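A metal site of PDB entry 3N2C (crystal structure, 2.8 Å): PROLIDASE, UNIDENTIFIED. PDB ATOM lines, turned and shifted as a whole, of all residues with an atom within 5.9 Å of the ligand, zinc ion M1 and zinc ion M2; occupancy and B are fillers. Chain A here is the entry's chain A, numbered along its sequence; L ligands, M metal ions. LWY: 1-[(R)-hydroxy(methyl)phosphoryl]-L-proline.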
ATOM      1  N   HIS A  65      -0.011  18.698  25.347  1.00  0.00           N
ATOM      2  CA  HIS A  65       0.040  17.588  24.409  1.00  0.00           C
ATOM      3  C   HIS A  65       0.383  18.030  22.993  1.00  0.00           C
ATOM      4  O   HIS A  65      -0.483  18.463  22.225  1.00  0.00           O
ATOM      5  CB  HIS A  65      -1.301  16.828  24.431  1.00  0.00           C
ATOM      6  CG  HIS A  65      -1.204  15.433  23.881  1.00  0.00           C
ATOM      7  ND1 HIS A  65      -1.277  14.311  24.688  1.00  0.00           N
ATOM      8  CD2 HIS A  65      -1.031  14.984  22.627  1.00  0.00           C
ATOM      9  CE1 HIS A  65      -1.165  13.226  23.931  1.00  0.00           C
ATOM     10  NE2 HIS A  65      -1.019  13.610  22.670  1.00  0.00           N
ATOM     11  N   VAL A  66       1.660  17.929  22.641  1.00  0.00           N
ATOM     12  CA  VAL A  66       2.106  18.212  21.277  1.00  0.00           C
ATOM     13  C   VAL A  66       2.899  17.056  20.668  1.00  0.00           C
ATOM     14  O   VAL A  66       3.358  16.144  21.364  1.00  0.00           O
ATOM     15  CB  VAL A  66       2.948  19.518  21.168  1.00  0.00           C
ATOM     16  CG1 VAL A  66       2.156  20.709  21.622  1.00  0.00           C
ATOM     17  CG2 VAL A  66       4.232  19.407  21.957  1.00  0.00           C
ATOM     18  N   HIS A  67       3.045  17.095  19.343  1.00  0.00           N
ATOM     19  CA  HIS A  67       3.974  16.234  18.635  1.00  0.00           C
ATOM     20  C   HIS A  67       4.795  17.096  17.702  1.00  0.00           C
ATOM     21  O   HIS A  67       4.488  17.236  16.517  1.00  0.00           O
ATOM     22  CB  HIS A  67       3.242  15.144  17.874  1.00  0.00           C
ATOM     23  CG  HIS A  67       2.688  14.071  18.741  1.00  0.00           C
ATOM     24  ND1 HIS A  67       3.485  13.304  19.571  1.00  0.00           N
ATOM     25  CD2 HIS A  67       1.431  13.630  18.916  1.00  0.00           C
ATOM     26  CE1 HIS A  67       2.728  12.441  20.230  1.00  0.00           C
ATOM     27  NE2 HIS A  67       1.472  12.616  19.836  1.00  0.00           N
ATOM     28  N   LEU A  75       1.648   9.338  10.519  1.00  0.00           N
ATOM     29  CA  LEU A  75       2.657   9.001  11.523  1.00  0.00           C
ATOM     30  C   LEU A  75       3.462   7.757  11.166  1.00  0.00           C
ATOM     31  O   LEU A  75       4.556   7.548  11.694  1.00  0.00           O
ATOM     32  CB  LEU A  75       2.023   8.831  12.902  1.00  0.00           C
ATOM     33  CG  LEU A  75       1.346  10.034  13.563  1.00  0.00           C
ATOM     34  CD1 LEU A  75       0.724   9.605  14.872  1.00  0.00           C
ATOM     35  CD2 LEU A  75       2.321  11.179  13.788  1.00  0.00           C
ATOM     36  N   ALA A 108       4.487  14.708  23.554  1.00  0.00           N
ATOM     37  CA  ALA A 108       3.849  13.446  23.901  1.00  0.00           C
ATOM     38  C   ALA A 108       4.452  12.251  23.175  1.00  0.00           C
ATOM     39  O   ALA A 108       3.873  11.171  23.175  1.00  0.00           O
ATOM     40  CB  ALA A 108       2.360  13.534  23.632  1.00  0.00           C
ATOM     41  N   HIS A 142      -0.877   1.193  19.601  1.00  0.00           N
ATOM     42  CA  HIS A 142      -1.105   2.487  18.966  1.00  0.00           C
ATOM     43  C   HIS A 142       0.176   3.096  18.388  1.00  0.00           C
ATOM     44  O   HIS A 142       0.118   3.928  17.471  1.00  0.00           O
ATOM     45  CB  HIS A 142      -1.787   3.452  19.950  1.00  0.00           C
ATOM     46  CG  HIS A 142      -2.286   4.717  19.311  1.00  0.00           C
ATOM     47  ND1 HIS A 142      -2.789   4.748  18.025  1.00  0.00           N
ATOM     48  CD2 HIS A 142      -2.360   5.986  19.770  1.00  0.00           C
ATOM     49  CE1 HIS A 142      -3.137   5.990  17.725  1.00  0.00           C
ATOM     50  NE2 HIS A 142      -2.905   6.750  18.769  1.00  0.00           N
ATOM     51  N   ILE A 164       7.408   8.680  16.688  1.00  0.00           N
ATOM     52  CA  ILE A 164       6.653   9.091  17.868  1.00  0.00           C
ATOM     53  C   ILE A 164       6.831   8.108  19.031  1.00  0.00           C
ATOM     54  O   ILE A 164       7.048   8.509  20.180  1.00  0.00           O
ATOM     55  CB  ILE A 164       5.135   9.235  17.528  1.00  0.00           C
ATOM     56  CG1 ILE A 164       4.925  10.170  16.323  1.00  0.00           C
ATOM     57  CG2 ILE A 164       4.320   9.681  18.730  1.00  0.00           C
ATOM     58  CD1 ILE A 164       5.398  11.610  16.528  1.00  0.00           C
ATOM     59  N   KCX A 190       5.492   8.527  28.439  1.00  0.00           N
ATOM     60  CA  KCX A 190       4.262   8.301  27.698  1.00  0.00           C
ATOM     61  CB  KCX A 190       4.303   9.016  26.351  1.00  0.00           C
ATOM     62  CG  KCX A 190       3.091   8.759  25.471  1.00  0.00           C
ATOM     63  CD  KCX A 190       1.837   9.401  26.057  1.00  0.00           C
ATOM     64  CE  KCX A 190       0.677   9.354  25.084  1.00  0.00           C
ATOM     65  NZ  KCX A 190       0.923  10.219  23.888  1.00  0.00           N
ATOM     66  C   KCX A 190       4.005   6.805  27.490  1.00  0.00           C
ATOM     67  O   KCX A 190       4.933   6.048  27.190  1.00  0.00           O
ATOM     68  CX  KCX A 190       0.072  10.213  22.878  1.00  0.00           C
ATOM     69  OQ1 KCX A 190      -0.933   9.477  22.911  1.00  0.00           O
ATOM     70  OQ2 KCX A 190       0.264  10.932  21.887  1.00  0.00           O
ATOM     71  N   MET A 192       0.819   4.024  25.634  1.00  0.00           N
ATOM     72  CA  MET A 192      -0.446   3.807  24.921  1.00  0.00           C
ATOM     73  C   MET A 192      -1.260   2.769  25.696  1.00  0.00           C
ATOM     74  O   MET A 192      -0.978   1.568  25.633  1.00  0.00           O
ATOM     75  CB  MET A 192      -0.189   3.323  23.490  1.00  0.00           C
ATOM     76  CG  MET A 192       0.759   4.186  22.675  1.00  0.00           C
ATOM     77  SD  MET A 192       0.119   5.824  22.320  1.00  0.00           S
ATOM     78  CE  MET A 192       1.307   6.405  21.111  1.00  0.00           C
ATOM     79  N   GLY A 195      -6.475   1.578  22.361  1.00  0.00           N
ATOM     80  CA  GLY A 195      -6.464   1.776  20.926  1.00  0.00           C
ATOM     81  C   GLY A 195      -6.562   3.245  20.565  1.00  0.00           C
ATOM     82  O   GLY A 195      -7.070   4.054  21.353  1.00  0.00           O
ATOM     83  N   GLY A 196      -6.071   3.604  19.389  1.00  0.00           N
ATOM     84  CA  GLY A 196      -6.117   4.976  18.932  1.00  0.00           C
ATOM     85  C   GLY A 196      -6.641   5.098  17.514  1.00  0.00           C
ATOM     86  O   GLY A 196      -7.073   4.121  16.902  1.00  0.00           O
ATOM     87  N   VAL A 197      -6.579   6.328  16.999  1.00  0.00           N
ATOM     88  CA  VAL A 197      -7.176   6.677  15.702  1.00  0.00           C
ATOM     89  C   VAL A 197      -6.152   6.572  14.559  1.00  0.00           C
ATOM     90  O   VAL A 197      -6.488   6.121  13.463  1.00  0.00           O
ATOM     91  CB  VAL A 197      -7.793   8.096  15.741  1.00  0.00           C
ATOM     92  CG1 VAL A 197      -8.641   8.346  14.538  1.00  0.00           C
ATOM     93  CG2 VAL A 197      -8.624   8.285  17.006  1.00  0.00           C
ATOM     94  N   ALA A 198      -4.911   6.955  14.844  1.00  0.00           N
ATOM     95  CA  ALA A 198      -3.834   7.030  13.837  1.00  0.00           C
ATOM     96  C   ALA A 198      -3.313   5.671  13.364  1.00  0.00           C
ATOM     97  O   ALA A 198      -3.104   5.474  12.161  1.00  0.00           O
ATOM     98  CB  ALA A 198      -2.690   7.909  14.342  1.00  0.00           C
ATOM     99  N   SER A 199      -3.083   4.760  14.300  1.00  0.00           N
ATOM    100  CA  SER A 199      -2.593   3.406  13.995  1.00  0.00           C
ATOM    101  C   SER A 199      -3.650   2.559  13.285  1.00  0.00           C
ATOM    102  O   SER A 199      -4.824   2.582  13.680  1.00  0.00           O
ATOM    103  CB  SER A 199      -2.144   2.709  15.288  1.00  0.00           C
ATOM    104  OG  SER A 199      -3.166   2.778  16.267  1.00  0.00           O
ATOM    105  N   ILE A 204     -10.357   1.750  18.759  1.00  0.00           N
ATOM    106  CA  ILE A 204     -10.277   2.637  19.932  1.00  0.00           C
ATOM    107  C   ILE A 204     -10.950   2.063  21.186  1.00  0.00           C
ATOM    108  O   ILE A 204     -10.680   2.521  22.311  1.00  0.00           O
ATOM    109  CB  ILE A 204     -10.877   4.045  19.622  1.00  0.00           C
ATOM    110  CG1 ILE A 204     -12.337   3.938  19.170  1.00  0.00           C
ATOM    111  CG2 ILE A 204     -10.040   4.770  18.579  1.00  0.00           C
ATOM    112  CD1 ILE A 204     -13.155   5.161  19.432  1.00  0.00           C
ATOM    113  N   HIS A 231      -2.337   7.577  27.016  1.00  0.00           N
ATOM    114  CA  HIS A 231      -3.341   7.692  25.966  1.00  0.00           C
ATOM    115  C   HIS A 231      -4.444   6.641  26.168  1.00  0.00           C
ATOM    116  O   HIS A 231      -4.190   5.437  26.127  1.00  0.00           O
ATOM    117  CB  HIS A 231      -2.641   7.553  24.604  1.00  0.00           C
ATOM    118  CG  HIS A 231      -3.518   7.100  23.490  1.00  0.00           C
ATOM    119  ND1 HIS A 231      -4.205   7.983  22.684  1.00  0.00           N
ATOM    120  CD2 HIS A 231      -3.807   5.862  23.009  1.00  0.00           C
ATOM    121  CE1 HIS A 231      -4.882   7.313  21.773  1.00  0.00           C
ATOM    122  NE2 HIS A 231      -4.664   6.024  21.951  1.00  0.00           N
ATOM    123  N   TYR A 233      -9.036   6.193  25.565  1.00  0.00           N
ATOM    124  CA  TYR A 233     -10.309   6.753  25.083  1.00  0.00           C
ATOM    125  C   TYR A 233     -11.511   6.362  25.938  1.00  0.00           C
ATOM    126  O   TYR A 233     -12.195   7.230  26.483  1.00  0.00           O
ATOM    127  CB  TYR A 233     -10.556   6.370  23.626  1.00  0.00           C
ATOM    128  CG  TYR A 233      -9.805   7.236  22.650  1.00  0.00           C
ATOM    129  CD1 TYR A 233     -10.058   8.597  22.577  1.00  0.00           C
ATOM    130  CD2 TYR A 233      -8.845   6.693  21.810  1.00  0.00           C
ATOM    131  CE1 TYR A 233      -9.382   9.404  21.682  1.00  0.00           C
ATOM    132  CE2 TYR A 233      -8.150   7.500  20.903  1.00  0.00           C
ATOM    133  CZ  TYR A 233      -8.422   8.855  20.851  1.00  0.00           C
ATOM    134  OH  TYR A 233      -7.752   9.667  19.972  1.00  0.00           O
ATOM    135  N   GLU A 250      -4.614  11.303  28.449  1.00  0.00           N
ATOM    136  CA  GLU A 250      -4.731  12.065  27.204  1.00  0.00           C
ATOM    137  C   GLU A 250      -6.064  11.756  26.541  1.00  0.00           C
ATOM    138  O   GLU A 250      -6.613  10.663  26.722  1.00  0.00           O
ATOM    139  CB  GLU A 250      -3.555  11.756  26.274  1.00  0.00           C
ATOM    140  CG  GLU A 250      -2.196  11.721  26.956  1.00  0.00           C
ATOM    141  CD  GLU A 250      -1.867  12.997  27.709  1.00  0.00           C
ATOM    142  OE1 GLU A 250      -2.077  14.101  27.167  1.00  0.00           O
ATOM    143  OE2 GLU A 250      -1.387  12.898  28.859  1.00  0.00           O
ATOM    144  N   HIS A 251      -6.562  12.726  25.776  1.00  0.00           N
ATOM    145  CA  HIS A 251      -7.831  12.639  25.016  1.00  0.00           C
ATOM    146  C   HIS A 251      -9.060  12.402  25.899  1.00  0.00           C
ATOM    147  O   HIS A 251      -9.819  13.331  26.175  1.00  0.00           O
ATOM    148  CB  HIS A 251      -7.742  11.612  23.882  1.00  0.00           C
ATOM    149  CG  HIS A 251      -6.418  11.607  23.189  1.00  0.00           C
ATOM    150  ND1 HIS A 251      -6.088  12.515  22.208  1.00  0.00           N
ATOM    151  CD2 HIS A 251      -5.332  10.812  23.348  1.00  0.00           C
ATOM    152  CE1 HIS A 251      -4.849  12.279  21.796  1.00  0.00           C
ATOM    153  NE2 HIS A 251      -4.374  11.247  22.475  1.00  0.00           N
ATOM    154  N   THR A 273      -7.873  16.777  23.808  1.00  0.00           N
ATOM    155  CA  THR A 273      -7.292  17.455  22.643  1.00  0.00           C
ATOM    156  C   THR A 273      -8.328  17.495  21.535  1.00  0.00           C
ATOM    157  O   THR A 273      -8.271  16.725  20.587  1.00  0.00           O
ATOM    158  CB  THR A 273      -6.015  16.730  22.135  1.00  0.00           C
ATOM    159  OG1 THR A 273      -6.331  15.372  21.802  1.00  0.00           O
ATOM    160  CG2 THR A 273      -4.907  16.731  23.174  1.00  0.00           C
ATOM    161  N   THR A 276      -7.918  18.568  17.264  1.00  0.00           N
ATOM    162  CA  THR A 276      -7.326  17.677  16.257  1.00  0.00           C
ATOM    163  C   THR A 276      -8.372  16.894  15.457  1.00  0.00           C
ATOM    164  O   THR A 276      -8.182  16.659  14.266  1.00  0.00           O
ATOM    165  CB  THR A 276      -6.201  16.773  16.844  1.00  0.00           C
ATOM    166  OG1 THR A 276      -5.607  15.997  15.791  1.00  0.00           O
ATOM    167  CG2 THR A 276      -6.707  15.843  17.930  1.00  0.00           C
ATOM    168  N   TYR A 277      -9.477  16.527  16.115  1.00  0.00           N
ATOM    169  CA  TYR A 277     -10.531  15.758  15.477  1.00  0.00           C
ATOM    170  C   TYR A 277     -11.355  16.621  14.530  1.00  0.00           C
ATOM    171  O   TYR A 277     -11.804  16.148  13.481  1.00  0.00           O
ATOM    172  CB  TYR A 277     -11.426  15.118  16.539  1.00  0.00           C
ATOM    173  CG  TYR A 277     -10.668  14.337  17.574  1.00  0.00           C
ATOM    174  CD1 TYR A 277     -10.059  13.118  17.259  1.00  0.00           C
ATOM    175  CD2 TYR A 277     -10.537  14.827  18.874  1.00  0.00           C
ATOM    176  CE1 TYR A 277      -9.341  12.407  18.208  1.00  0.00           C
ATOM    177  CE2 TYR A 277      -9.828  14.112  19.834  1.00  0.00           C
ATOM    178  CZ  TYR A 277      -9.232  12.898  19.498  1.00  0.00           C
ATOM    179  OH  TYR A 277      -8.533  12.197  20.442  1.00  0.00           O
ATOM    180  N   LEU A 280      -9.146  16.979  11.536  1.00  0.00           N
ATOM    181  CA  LEU A 280      -9.188  15.724  10.769  1.00  0.00           C
ATOM    182  C   LEU A 280     -10.587  15.412  10.211  1.00  0.00           C
ATOM    183  O   LEU A 280     -10.754  14.469   9.441  1.00  0.00           O
ATOM    184  CB  LEU A 280      -8.669  14.551  11.607  1.00  0.00           C
ATOM    185  CG  LEU A 280      -7.180  14.543  11.985  1.00  0.00           C
ATOM    186  CD1 LEU A 280      -6.888  13.454  13.009  1.00  0.00           C
ATOM    187  CD2 LEU A 280      -6.283  14.416  10.759  1.00  0.00           C
ATOM    188  N   ASP A 323      -2.518  18.317  20.030  1.00  0.00           N
ATOM    189  CA  ASP A 323      -2.258  17.025  19.353  1.00  0.00           C
ATOM    190  C   ASP A 323      -2.383  17.102  17.819  1.00  0.00           C
ATOM    191  O   ASP A 323      -2.835  16.162  17.161  1.00  0.00           O
ATOM    192  CB  ASP A 323      -3.152  15.930  19.951  1.00  0.00           C
ATOM    193  CG  ASP A 323      -2.693  14.522  19.613  1.00  0.00           C
ATOM    194  OD1 ASP A 323      -1.469  14.250  19.686  1.00  0.00           O
ATOM    195  OD2 ASP A 323      -3.551  13.688  19.275  1.00  0.00           O
ATOM    196  N   LEU A 325      -1.107  17.400  13.853  1.00  0.00           N
ATOM    197  CA  LEU A 325      -0.042  16.786  13.062  1.00  0.00           C
ATOM    198  C   LEU A 325       0.148  17.526  11.741  1.00  0.00           C
ATOM    199  O   LEU A 325      -0.824  17.915  11.088  1.00  0.00           O
ATOM    200  CB  LEU A 325      -0.359  15.307  12.784  1.00  0.00           C
ATOM    201  CG  LEU A 325      -0.973  14.440  13.876  1.00  0.00           C
ATOM    202  CD1 LEU A 325      -1.602  13.201  13.268  1.00  0.00           C
ATOM    203  CD2 LEU A 325       0.018  14.054  14.968  1.00  0.00           C
HETATM  204  C   LWY L   1      -5.085   9.143  18.083  1.00  0.00           C
HETATM  205  N   LWY L   1      -3.455  10.972  17.821  1.00  0.00           N
HETATM  206  OXT LWY L   1      -5.750   8.497  18.913  1.00  0.00           O
HETATM  207  P   LWY L   1      -2.020  10.529  18.552  1.00  0.00           P
HETATM  208  C1  LWY L   1      -0.710  11.266  17.712  1.00  0.00           C
HETATM  209  O1  LWY L   1      -1.843   8.948  18.368  1.00  0.00           O
HETATM  210  O2  LWY L   1      -2.021  11.081  19.952  1.00  0.00           O
HETATM  211  CA  LWY L   1      -4.754  10.584  18.373  1.00  0.00           C
HETATM  212  CB  LWY L   1      -5.738  11.508  17.667  1.00  0.00           C
HETATM  213  CD  LWY L   1      -3.537  11.769  16.598  1.00  0.00           C
HETATM  214  CG  LWY L   1      -4.990  12.221  16.559  1.00  0.00           C
HETATM  215  O   LWY L   1      -4.670   8.638  17.026  1.00  0.00           O
HETATM  216 ZN    ZN M   1      -2.587   9.471  21.604  1.00  0.00          ZN
HETATM  217 ZN    ZN M   2      -0.436  12.483  20.935  1.00  0.00          ZN
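OQ1 of KCX 190 is bound to zinc ion M1 (2.1 Å).
O2 of the ligand binds zinc ion M1 (2.4 Å).
A ring nitrogen (ND1) of His 231 is bound to zinc ion M1, 2.4 Å away.
Zinc ion M1 is bound by NE2 of His 251, at 2.7 Å.
Zinc ion M1 has four donor atoms within binding distance.
Residues that only touch the ligand: Gly 196 (3.5 Å), Leu 75 (3.6 Å), Tyr 277 (3.8 Å), Thr 276 (3.9 Å) and Leu 325 (3.98 Å).
Hydrophobic or aromatic side chains that line the ligand: His 67, Leu 75, His 142, Val 197, Ala 198, His 231, Tyr 233, His 251, Tyr 277 and Leu 325.
Of the 25 residues printed, 15 come within 4 Å of the ligand.
Zinc ion M2 is bound by OQ2 of KCX 190, at 1.9 Å.
NE2 of His 65 binds zinc ion M2 (2.1 Å).
NE2 of His 67 binds zinc ion M2, at 2.2 Å.
An oxygen (O2) of the ligand binds zinc ion M2 (2.3 Å).
The side-chain carboxylate (OD1) of Asp 323 binds zinc ion M2, 2.4 Å away.
Zinc ion M2 has five donor atoms within binding distance.
Of the 25 residues printed, 4 come within 4 Å of zinc ion M2.
Along chain A the residues within 4 Å of zinc ion M2 span positions 65 to 323.
O1 of the ligand is in hydrogen-bond range of NE2 of His 142 (2.5 Å).
The side-chain hydroxyl of Tyr 233 is in hydrogen-bond range of an oxygen (OXT) of the ligand (2.5 Å).
N of Ala 198 lies within hydrogen-bond range of O of the ligand (2.8 Å).
O of the ligand lies within hydrogen-bond range of N of Val 197, 3.0 Å away.
His 142 touches zinc ion M1.
Within 4 Å of zinc ion M1: His 142, KCX 190, His 231 and His 251.
O of Ala 108 lies within hydrogen-bond range of NZ of KCX 190 (3.2 Å).
A ring nitrogen (ND1) of His 65 sits at hydrogen-bond distance from the side-chain carboxylate (OE1) of Glu 250, at 2.6 Å.
O of Asp 323 is in hydrogen-bond range of OG1 of Thr 276 (3.1 Å).
A ring nitrogen (NE2) of His 231 lies within hydrogen-bond range of the backbone carbonyl oxygen (O) of Gly 195 (3.2 Å).
A ring nitrogen (ND1) of His 142 sits at hydrogen-bond distance from the side-chain hydroxyl (OG) of Ser 199, at 2.7 Å.
OH of Tyr 233 is in hydrogen-bond range of OH of Tyr 277.
OH of Tyr 277 sits at hydrogen-bond distance from ND1 of His 251.
A ring nitrogen (ND1) of His 251 is in hydrogen-bond range of the side-chain hydroxyl (OG1) of Thr 273.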
